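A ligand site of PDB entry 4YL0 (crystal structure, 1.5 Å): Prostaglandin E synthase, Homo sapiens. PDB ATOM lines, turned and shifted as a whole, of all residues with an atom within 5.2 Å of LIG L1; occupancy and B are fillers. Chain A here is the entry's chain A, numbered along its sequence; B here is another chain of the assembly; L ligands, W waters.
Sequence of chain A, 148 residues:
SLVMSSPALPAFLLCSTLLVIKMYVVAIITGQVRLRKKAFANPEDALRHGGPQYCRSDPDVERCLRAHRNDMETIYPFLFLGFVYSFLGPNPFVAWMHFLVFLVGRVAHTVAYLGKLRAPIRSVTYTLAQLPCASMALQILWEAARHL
OH of Tyr 113 lies within hydrogen-bond range of O6 of LIG L1 (2.6 Å). A ring nitrogen (NE2) of His 109 is in hydrogen-bond range of an oxygen (O4) of LIG L1 (2.9 Å). The side-chain amide nitrogen of Asn 70 is in hydrogen-bond range of an oxygen (O3) of LIG L1, at 2.9 Å. An oxygen (O4) of LIG L1 lies within hydrogen-bond range of the guanidinium group (NE) of Arg 122, 2.9 Å away. The side-chain hydroxyl (OG) of Ser 123 sits close to a sulfur (S1) of LIG L1 (3.0 Å). The side-chain carboxylate (OE1) of Glu 73 lies within salt-bridge range of a nitrogen (N1) of LIG L1, at 3.0 Å. The guanidinium group (NE) of Arg 34 of chain B is in salt-bridge range of an oxygen (O2) of LIG L1 (3.1 Å). N1 of LG2 L2 sits close to OG of Ser 123 (3.4 Å).
OH of Tyr 113 is in hydrogen-bond range of NE of Arg 66, 3.1 Å away. ND2 of Asn 42 of chain B is in hydrogen-bond range of OH of Tyr 113 (3.1 Å). NE2 of His 109 lies close to OD1 of Asn 70 (3.4 Å). NH2 of Arg 66 sits at hydrogen-bond distance from OD1 of Asn 42 of chain B, 2.8 Å away. O of Ala 41 of chain B lies within hydrogen-bond range of NH2 of Arg 66 (3.4 Å).
Residues that only touch LIG L1: Arg 66, Tyr 126, Ala 27 of chain B, Thr 30 of chain B and Leu 65 of chain B. Within 4 Å of LIG L1: Arg 66, Asn 70, Glu 73, His 109, Tyr 113, Arg 122, Ser 123, Tyr 126, Ala 27 of chain B, Thr 30 of chain B, Arg 34 of chain B and Leu 65 of chain B. The nearest printed residue that does not touch LIG L1 is His 68 of chain B (4.3 Å).
Water W3 lies within hydrogen-bond range of N1 of LIG L1, ND1 of His 68 of chain B and OG1 of Thr 30 of chain B. Water W4 lies within hydrogen-bond range of OE1 of Glu 73 and O3 of LIG L1. Water W5 lies within hydrogen-bond range of the guanidinium group of Arg 34 of chain B and an oxygen (O6) of LIG L1. Water W2 lies within hydrogen-bond range of a nitrogen (N1) of LG2 L2 and a sulfur (S1) of LIG L1. Water W6 lies within hydrogen-bond range of O6 of LIG L1 (3.2 Å) and NH2 of Arg 34 of chain B (3.3 Å).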
ATOM      1  N   ARG A  66      28.312  14.465  -0.942  1.00  0.00           N
ATOM      2  CA  ARG A  66      27.417  13.313  -0.969  1.00  0.00           C
ATOM      3  C   ARG A  66      26.727  13.160  -2.315  1.00  0.00           C
ATOM      4  O   ARG A  66      26.594  12.040  -2.809  1.00  0.00           O
ATOM      5  CB  ARG A  66      26.374  13.359   0.161  1.00  0.00           C
ATOM      6  CG  ARG A  66      26.961  13.095   1.538  1.00  0.00           C
ATOM      7  CD  ARG A  66      25.893  12.811   2.594  1.00  0.00           C
ATOM      8  NE  ARG A  66      24.961  13.938   2.789  1.00  0.00           N
ATOM      9  CZ  ARG A  66      25.223  15.011   3.533  1.00  0.00           C
ATOM     10  NH1 ARG A  66      26.368  15.120   4.195  1.00  0.00           N
ATOM     11  NH2 ARG A  66      24.311  15.978   3.637  1.00  0.00           N
ATOM     12  N   ASN A  70      27.213   9.987  -4.681  1.00  0.00           N
ATOM     13  CA  ASN A  70      26.098   9.190  -5.184  1.00  0.00           C
ATOM     14  C   ASN A  70      26.083   9.107  -6.714  1.00  0.00           C
ATOM     15  O   ASN A  70      25.784   8.047  -7.282  1.00  0.00           O
ATOM     16  CB  ASN A  70      24.768   9.707  -4.634  1.00  0.00           C
ATOM     17  CG  ASN A  70      23.640   8.731  -4.872  1.00  0.00           C
ATOM     18  OD1 ASN A  70      22.990   8.776  -5.906  1.00  0.00           O
ATOM     19  ND2 ASN A  70      23.433   7.819  -3.922  1.00  0.00           N
ATOM     20  N   GLU A  73      28.506   6.493  -7.677  1.00  0.00           N
ATOM     21  CA  GLU A  73      27.956   5.176  -7.348  1.00  0.00           C
ATOM     22  C   GLU A  73      26.964   4.692  -8.397  1.00  0.00           C
ATOM     23  O   GLU A  73      26.719   3.489  -8.511  1.00  0.00           O
ATOM     24  CB  GLU A  73      27.303   5.191  -5.953  1.00  0.00           C
ATOM     25  CG  GLU A  73      28.299   5.407  -4.810  1.00  0.00           C
ATOM     26  CD  GLU A  73      27.659   5.631  -3.446  1.00  0.00           C
ATOM     27  OE1 GLU A  73      26.430   5.650  -3.336  1.00  0.00           O
ATOM     28  OE2 GLU A  73      28.426   5.793  -2.464  1.00  0.00           O
ATOM     29  N   HIS A 109      17.539  13.756  -9.142  1.00  0.00           N
ATOM     30  CA  HIS A 109      18.272  13.397  -7.912  1.00  0.00           C
ATOM     31  C   HIS A 109      19.179  14.537  -7.436  1.00  0.00           C
ATOM     32  O   HIS A 109      19.157  14.891  -6.256  1.00  0.00           O
ATOM     33  CB  HIS A 109      19.105  12.129  -8.132  1.00  0.00           C
ATOM     34  CG  HIS A 109      19.724  11.594  -6.871  1.00  0.00           C
ATOM     35  ND1 HIS A 109      20.949  12.014  -6.405  1.00  0.00           N
ATOM     36  CD2 HIS A 109      19.273  10.673  -5.993  1.00  0.00           C
ATOM     37  CE1 HIS A 109      21.232  11.372  -5.286  1.00  0.00           C
ATOM     38  NE2 HIS A 109      20.236  10.547  -5.015  1.00  0.00           N
ATOM     39  N   TYR A 113      18.761  16.683  -4.133  1.00  0.00           N
ATOM     40  CA  TYR A 113      19.831  16.622  -3.135  1.00  0.00           C
ATOM     41  C   TYR A 113      20.327  18.023  -2.783  1.00  0.00           C
ATOM     42  O   TYR A 113      20.293  18.423  -1.620  1.00  0.00           O
ATOM     43  CB  TYR A 113      21.003  15.750  -3.612  1.00  0.00           C
ATOM     44  CG  TYR A 113      21.632  14.938  -2.497  1.00  0.00           C
ATOM     45  CD1 TYR A 113      21.479  15.308  -1.164  1.00  0.00           C
ATOM     46  CD2 TYR A 113      22.358  13.776  -2.786  1.00  0.00           C
ATOM     47  CE1 TYR A 113      22.035  14.555  -0.134  1.00  0.00           C
ATOM     48  CE2 TYR A 113      22.907  13.012  -1.762  1.00  0.00           C
ATOM     49  CZ  TYR A 113      22.737  13.408  -0.438  1.00  0.00           C
ATOM     50  OH  TYR A 113      23.270  12.659   0.590  1.00  0.00           O
ATOM     51  N   ARG A 122      14.198  12.596  -3.044  1.00  0.00           N
ATOM     52  CA  ARG A 122      15.509  12.147  -3.522  1.00  0.00           C
ATOM     53  C   ARG A 122      15.591  10.621  -3.618  1.00  0.00           C
ATOM     54  O   ARG A 122      16.058  10.086  -4.627  1.00  0.00           O
ATOM     55  CB  ARG A 122      16.630  12.696  -2.635  1.00  0.00           C
ATOM     56  CG  ARG A 122      18.027  12.469  -3.202  1.00  0.00           C
ATOM     57  CD  ARG A 122      19.100  12.670  -2.149  1.00  0.00           C
ATOM     58  NE  ARG A 122      19.120  11.571  -1.187  1.00  0.00           N
ATOM     59  CZ  ARG A 122      18.656  11.633   0.065  1.00  0.00           C
ATOM     60  NH1 ARG A 122      18.155  12.758   0.557  1.00  0.00           N
ATOM     61  NH2 ARG A 122      18.731  10.554   0.829  1.00  0.00           N
ATOM     62  N   SER A 123      15.123   9.922  -2.574  1.00  0.00           N
ATOM     63  CA  SER A 123      15.118   8.463  -2.535  1.00  0.00           C
ATOM     64  C   SER A 123      14.341   7.865  -3.702  1.00  0.00           C
ATOM     65  O   SER A 123      14.774   6.870  -4.294  1.00  0.00           O
ATOM     66  CB  SER A 123      14.541   7.953  -1.219  1.00  0.00           C
ATOM     67  OG  SER A 123      15.382   8.330  -0.143  1.00  0.00           O
ATOM     68  N   TYR A 126      16.303   8.302  -6.977  1.00  0.00           N
ATOM     69  CA  TYR A 126      17.383   7.316  -6.999  1.00  0.00           C
ATOM     70  C   TYR A 126      16.849   5.961  -7.463  1.00  0.00           C
ATOM     71  O   TYR A 126      17.425   5.324  -8.351  1.00  0.00           O
ATOM     72  CB  TYR A 126      18.040   7.197  -5.620  1.00  0.00           C
ATOM     73  CG  TYR A 126      18.878   5.962  -5.427  1.00  0.00           C
ATOM     74  CD1 TYR A 126      20.219   5.916  -5.847  1.00  0.00           C
ATOM     75  CD2 TYR A 126      18.348   4.825  -4.812  1.00  0.00           C
ATOM     76  CE1 TYR A 126      20.989   4.772  -5.675  1.00  0.00           C
ATOM     77  CE2 TYR A 126      19.104   3.682  -4.630  1.00  0.00           C
ATOM     78  CZ  TYR A 126      20.414   3.660  -5.058  1.00  0.00           C
ATOM     79  OH  TYR A 126      21.157   2.519  -4.866  1.00  0.00           O
ATOM     80  N   ALA B  27      24.818  -1.127  -2.048  1.00  0.00           N
ATOM     81  CA  ALA B  27      24.009   0.090  -1.917  1.00  0.00           C
ATOM     82  C   ALA B  27      22.677  -0.179  -1.217  1.00  0.00           C
ATOM     83  O   ALA B  27      22.256   0.602  -0.358  1.00  0.00           O
ATOM     84  CB  ALA B  27      23.765   0.749  -3.275  1.00  0.00           C
ATOM     85  N   THR B  30      23.317  -0.843   2.445  1.00  0.00           N
ATOM     86  CA  THR B  30      23.601   0.447   3.091  1.00  0.00           C
ATOM     87  C   THR B  30      22.314   1.173   3.492  1.00  0.00           C
ATOM     88  O   THR B  30      22.187   1.640   4.621  1.00  0.00           O
ATOM     89  CB  THR B  30      24.472   1.364   2.204  1.00  0.00           C
ATOM     90  OG1 THR B  30      25.662   0.678   1.799  1.00  0.00           O
ATOM     91  CG2 THR B  30      24.863   2.628   2.955  1.00  0.00           C
ATOM     92  N   GLY B  31      21.359   1.256   2.562  1.00  0.00           N
ATOM     93  CA  GLY B  31      20.070   1.884   2.838  1.00  0.00           C
ATOM     94  C   GLY B  31      19.307   1.173   3.950  1.00  0.00           C
ATOM     95  O   GLY B  31      18.716   1.816   4.815  1.00  0.00           O
ATOM     96  N   ARG B  34      20.904   2.014   7.290  1.00  0.00           N
ATOM     97  CA  ARG B  34      20.496   3.364   7.682  1.00  0.00           C
ATOM     98  C   ARG B  34      19.104   3.368   8.318  1.00  0.00           C
ATOM     99  O   ARG B  34      18.907   3.982   9.352  1.00  0.00           O
ATOM    100  CB  ARG B  34      20.510   4.327   6.492  1.00  0.00           C
ATOM    101  CG  ARG B  34      21.894   4.721   6.002  1.00  0.00           C
ATOM    102  CD  ARG B  34      21.771   5.906   5.041  1.00  0.00           C
ATOM    103  NE  ARG B  34      23.069   6.372   4.547  1.00  0.00           N
ATOM    104  CZ  ARG B  34      23.900   7.158   5.223  1.00  0.00           C
ATOM    105  NH1 ARG B  34      23.605   7.560   6.460  1.00  0.00           N
ATOM    106  NH2 ARG B  34      25.039   7.546   4.671  1.00  0.00           N
ATOM    107  N   ALA B  41      22.158  10.575   6.708  1.00  0.00           N
ATOM    108  CA  ALA B  41      23.146  11.594   6.389  1.00  0.00           C
ATOM    109  C   ALA B  41      22.554  12.986   6.193  1.00  0.00           C
ATOM    110  O   ALA B  41      23.287  13.990   6.219  1.00  0.00           O
ATOM    111  CB  ALA B  41      23.942  11.169   5.171  1.00  0.00           C
ATOM    112  N   ASN B  42      21.237  13.062   6.029  1.00  0.00           N
ATOM    113  CA  ASN B  42      20.563  14.304   5.674  1.00  0.00           C
ATOM    114  C   ASN B  42      19.441  14.631   6.641  1.00  0.00           C
ATOM    115  O   ASN B  42      18.668  13.743   6.998  1.00  0.00           O
ATOM    116  CB  ASN B  42      19.993  14.201   4.257  1.00  0.00           C
ATOM    117  CG  ASN B  42      21.056  13.878   3.236  1.00  0.00           C
ATOM    118  OD1 ASN B  42      21.940  14.698   2.988  1.00  0.00           O
ATOM    119  ND2 ASN B  42      20.990  12.695   2.647  1.00  0.00           N
ATOM    120  N   LEU B  65      29.725   2.139   3.657  1.00  0.00           N
ATOM    121  CA  LEU B  65      30.249   3.169   2.761  1.00  0.00           C
ATOM    122  C   LEU B  65      31.700   2.907   2.376  1.00  0.00           C
ATOM    123  O   LEU B  65      32.086   3.138   1.233  1.00  0.00           O
ATOM    124  CB  LEU B  65      30.085   4.578   3.365  1.00  0.00           C
ATOM    125  CG  LEU B  65      28.646   5.094   3.502  1.00  0.00           C
ATOM    126  CD1 LEU B  65      28.616   6.390   4.294  1.00  0.00           C
ATOM    127  CD2 LEU B  65      27.982   5.296   2.147  1.00  0.00           C
ATOM    128  N   HIS B  68      31.719   0.083  -0.231  1.00  0.00           N
ATOM    129  CA  HIS B  68      31.240   0.627  -1.516  1.00  0.00           C
ATOM    130  C   HIS B  68      32.333   1.490  -2.140  1.00  0.00           C
ATOM    131  O   HIS B  68      32.590   1.388  -3.346  1.00  0.00           O
ATOM    132  CB  HIS B  68      29.933   1.411  -1.305  1.00  0.00           C
ATOM    133  CG  HIS B  68      29.108   1.558  -2.545  1.00  0.00           C
ATOM    134  ND1 HIS B  68      27.807   2.015  -2.515  1.00  0.00           N
ATOM    135  CD2 HIS B  68      29.383   1.308  -3.857  1.00  0.00           C
ATOM    136  CE1 HIS B  68      27.322   2.042  -3.745  1.00  0.00           C
ATOM    137  NE2 HIS B  68      28.261   1.618  -4.582  1.00  0.00           N
HETATM  138  N1  LIG L   1      25.747   5.176  -0.409  1.00  0.00           N
HETATM  139  C1  LIG L   1      24.266   5.325  -0.377  1.00  0.00           C
HETATM  140  C2  LIG L   1      23.788   5.929   0.916  1.00  0.00           C
HETATM  141  O1  LIG L   1      22.609   6.331   1.007  1.00  0.00           O
HETATM  142  O2  LIG L   1      24.584   6.020   1.881  1.00  0.00           O
HETATM  143  C3  LIG L   1      23.632   3.960  -0.688  1.00  0.00           C
HETATM  144  C4  LIG L   1      22.128   3.956  -0.952  1.00  0.00           C
HETATM  145  C5  LIG L   1      21.692   5.107  -1.837  1.00  0.00           C
HETATM  146  O3  LIG L   1      22.313   5.393  -2.840  1.00  0.00           O
HETATM  147  N2  LIG L   1      20.610   5.784  -1.429  1.00  0.00           N
HETATM  148  C6  LIG L   1      20.034   6.900  -2.174  1.00  0.00           C
HETATM  149  C7  LIG L   1      20.677   8.236  -1.884  1.00  0.00           C
HETATM  150  O4  LIG L   1      20.296   9.239  -2.483  1.00  0.00           O
HETATM  151  C8  LIG L   1      18.527   6.982  -1.895  1.00  0.00           C
HETATM  152  S1  LIG L   1      18.161   7.295  -0.160  1.00  0.00           S
HETATM  153  N3  LIG L   1      21.651   8.242  -0.963  1.00  0.00           N
HETATM  154  C9  LIG L   1      22.254   9.483  -0.502  1.00  0.00           C
HETATM  155  C10 LIG L   1      23.750   9.460  -0.526  1.00  0.00           C
HETATM  156  O5  LIG L   1      24.333   8.525  -1.128  1.00  0.00           O
HETATM  157  O6  LIG L   1      24.357  10.380   0.071  1.00  0.00           O
HETATM  158  C1  LG2 L   2      17.203   7.522   3.664  1.00  0.00           C
HETATM  159  C2  LG2 L   2      17.655   5.157   3.420  1.00  0.00           C
HETATM  160  C3  LG2 L   2      16.012   3.630   2.508  1.00  0.00           C
HETATM  161  C4  LG2 L   2      18.073   6.432   3.806  1.00  0.00           C
HETATM  162  C5  LG2 L   2       8.685   6.809   2.997  1.00  0.00           C
HETATM  163  C6  LG2 L   2       7.898   6.508   1.884  1.00  0.00           C
HETATM  164  C7  LG2 L   2      15.094   8.502   3.021  1.00  0.00           C
HETATM  165 CL1  LG2 L   2       9.680   4.061  -4.337  1.00  0.00          CL
HETATM  166  C8  LG2 L   2      10.560   4.462  -2.909  1.00  0.00           C
HETATM  167  C9  LG2 L   2      11.938   4.299  -2.883  1.00  0.00           C
HETATM  168  C10 LG2 L   2       9.875   4.950  -1.787  1.00  0.00           C
HETATM  169  C11 LG2 L   2      10.538   5.305  -0.587  1.00  0.00           C
HETATM  170  C12 LG2 L   2       9.882   5.805   0.604  1.00  0.00           C
HETATM  171  C13 LG2 L   2       8.482   6.020   0.709  1.00  0.00           C
HETATM  172  C14 LG2 L   2      11.959   5.122  -0.587  1.00  0.00           C
HETATM  173  C15 LG2 L   2      12.645   4.628  -1.727  1.00  0.00           C
HETATM  174  C16 LG2 L   2      12.680   5.457   0.578  1.00  0.00           C
HETATM  175  N1  LG2 L   2      14.022   5.403   0.905  1.00  0.00           N
HETATM  176  C17 LG2 L   2      14.181   5.844   2.181  1.00  0.00           C
HETATM  177  C18 LG2 L   2      15.496   6.058   2.741  1.00  0.00           C
HETATM  178  C19 LG2 L   2      15.920   7.344   3.134  1.00  0.00           C
HETATM  179  N2  LG2 L   2      14.419   9.442   2.921  1.00  0.00           N
HETATM  180  C20 LG2 L   2      16.374   4.966   2.894  1.00  0.00           C
HETATM  181  N3  LG2 L   2      15.738   2.555   2.189  1.00  0.00           N
HETATM  182  N4  LG2 L   2      13.020   6.174   2.722  1.00  0.00           N
HETATM  183  C21 LG2 L   2      12.074   5.946   1.742  1.00  0.00           C
HETATM  184  C22 LG2 L   2      10.668   6.123   1.765  1.00  0.00           C
HETATM  185  C23 LG2 L   2      10.063   6.616   2.938  1.00  0.00           C
HETATM  186  O   HOH W   1      20.702   7.693   2.223  1.00  0.00           O
HETATM  187  O   HOH W   2      16.329   4.735  -0.578  1.00  0.00           O
HETATM  188  O   HOH W   3      26.728   2.673  -0.053  1.00  0.00           O
HETATM  189  O   HOH W   4      24.333   4.242  -4.417  1.00  0.00           O
HETATM  190  O   HOH W   5      25.895   9.080   2.356  1.00  0.00           O
HETATM  191  O   HOH W   6      22.929   9.266   2.747  1.00  0.00           O
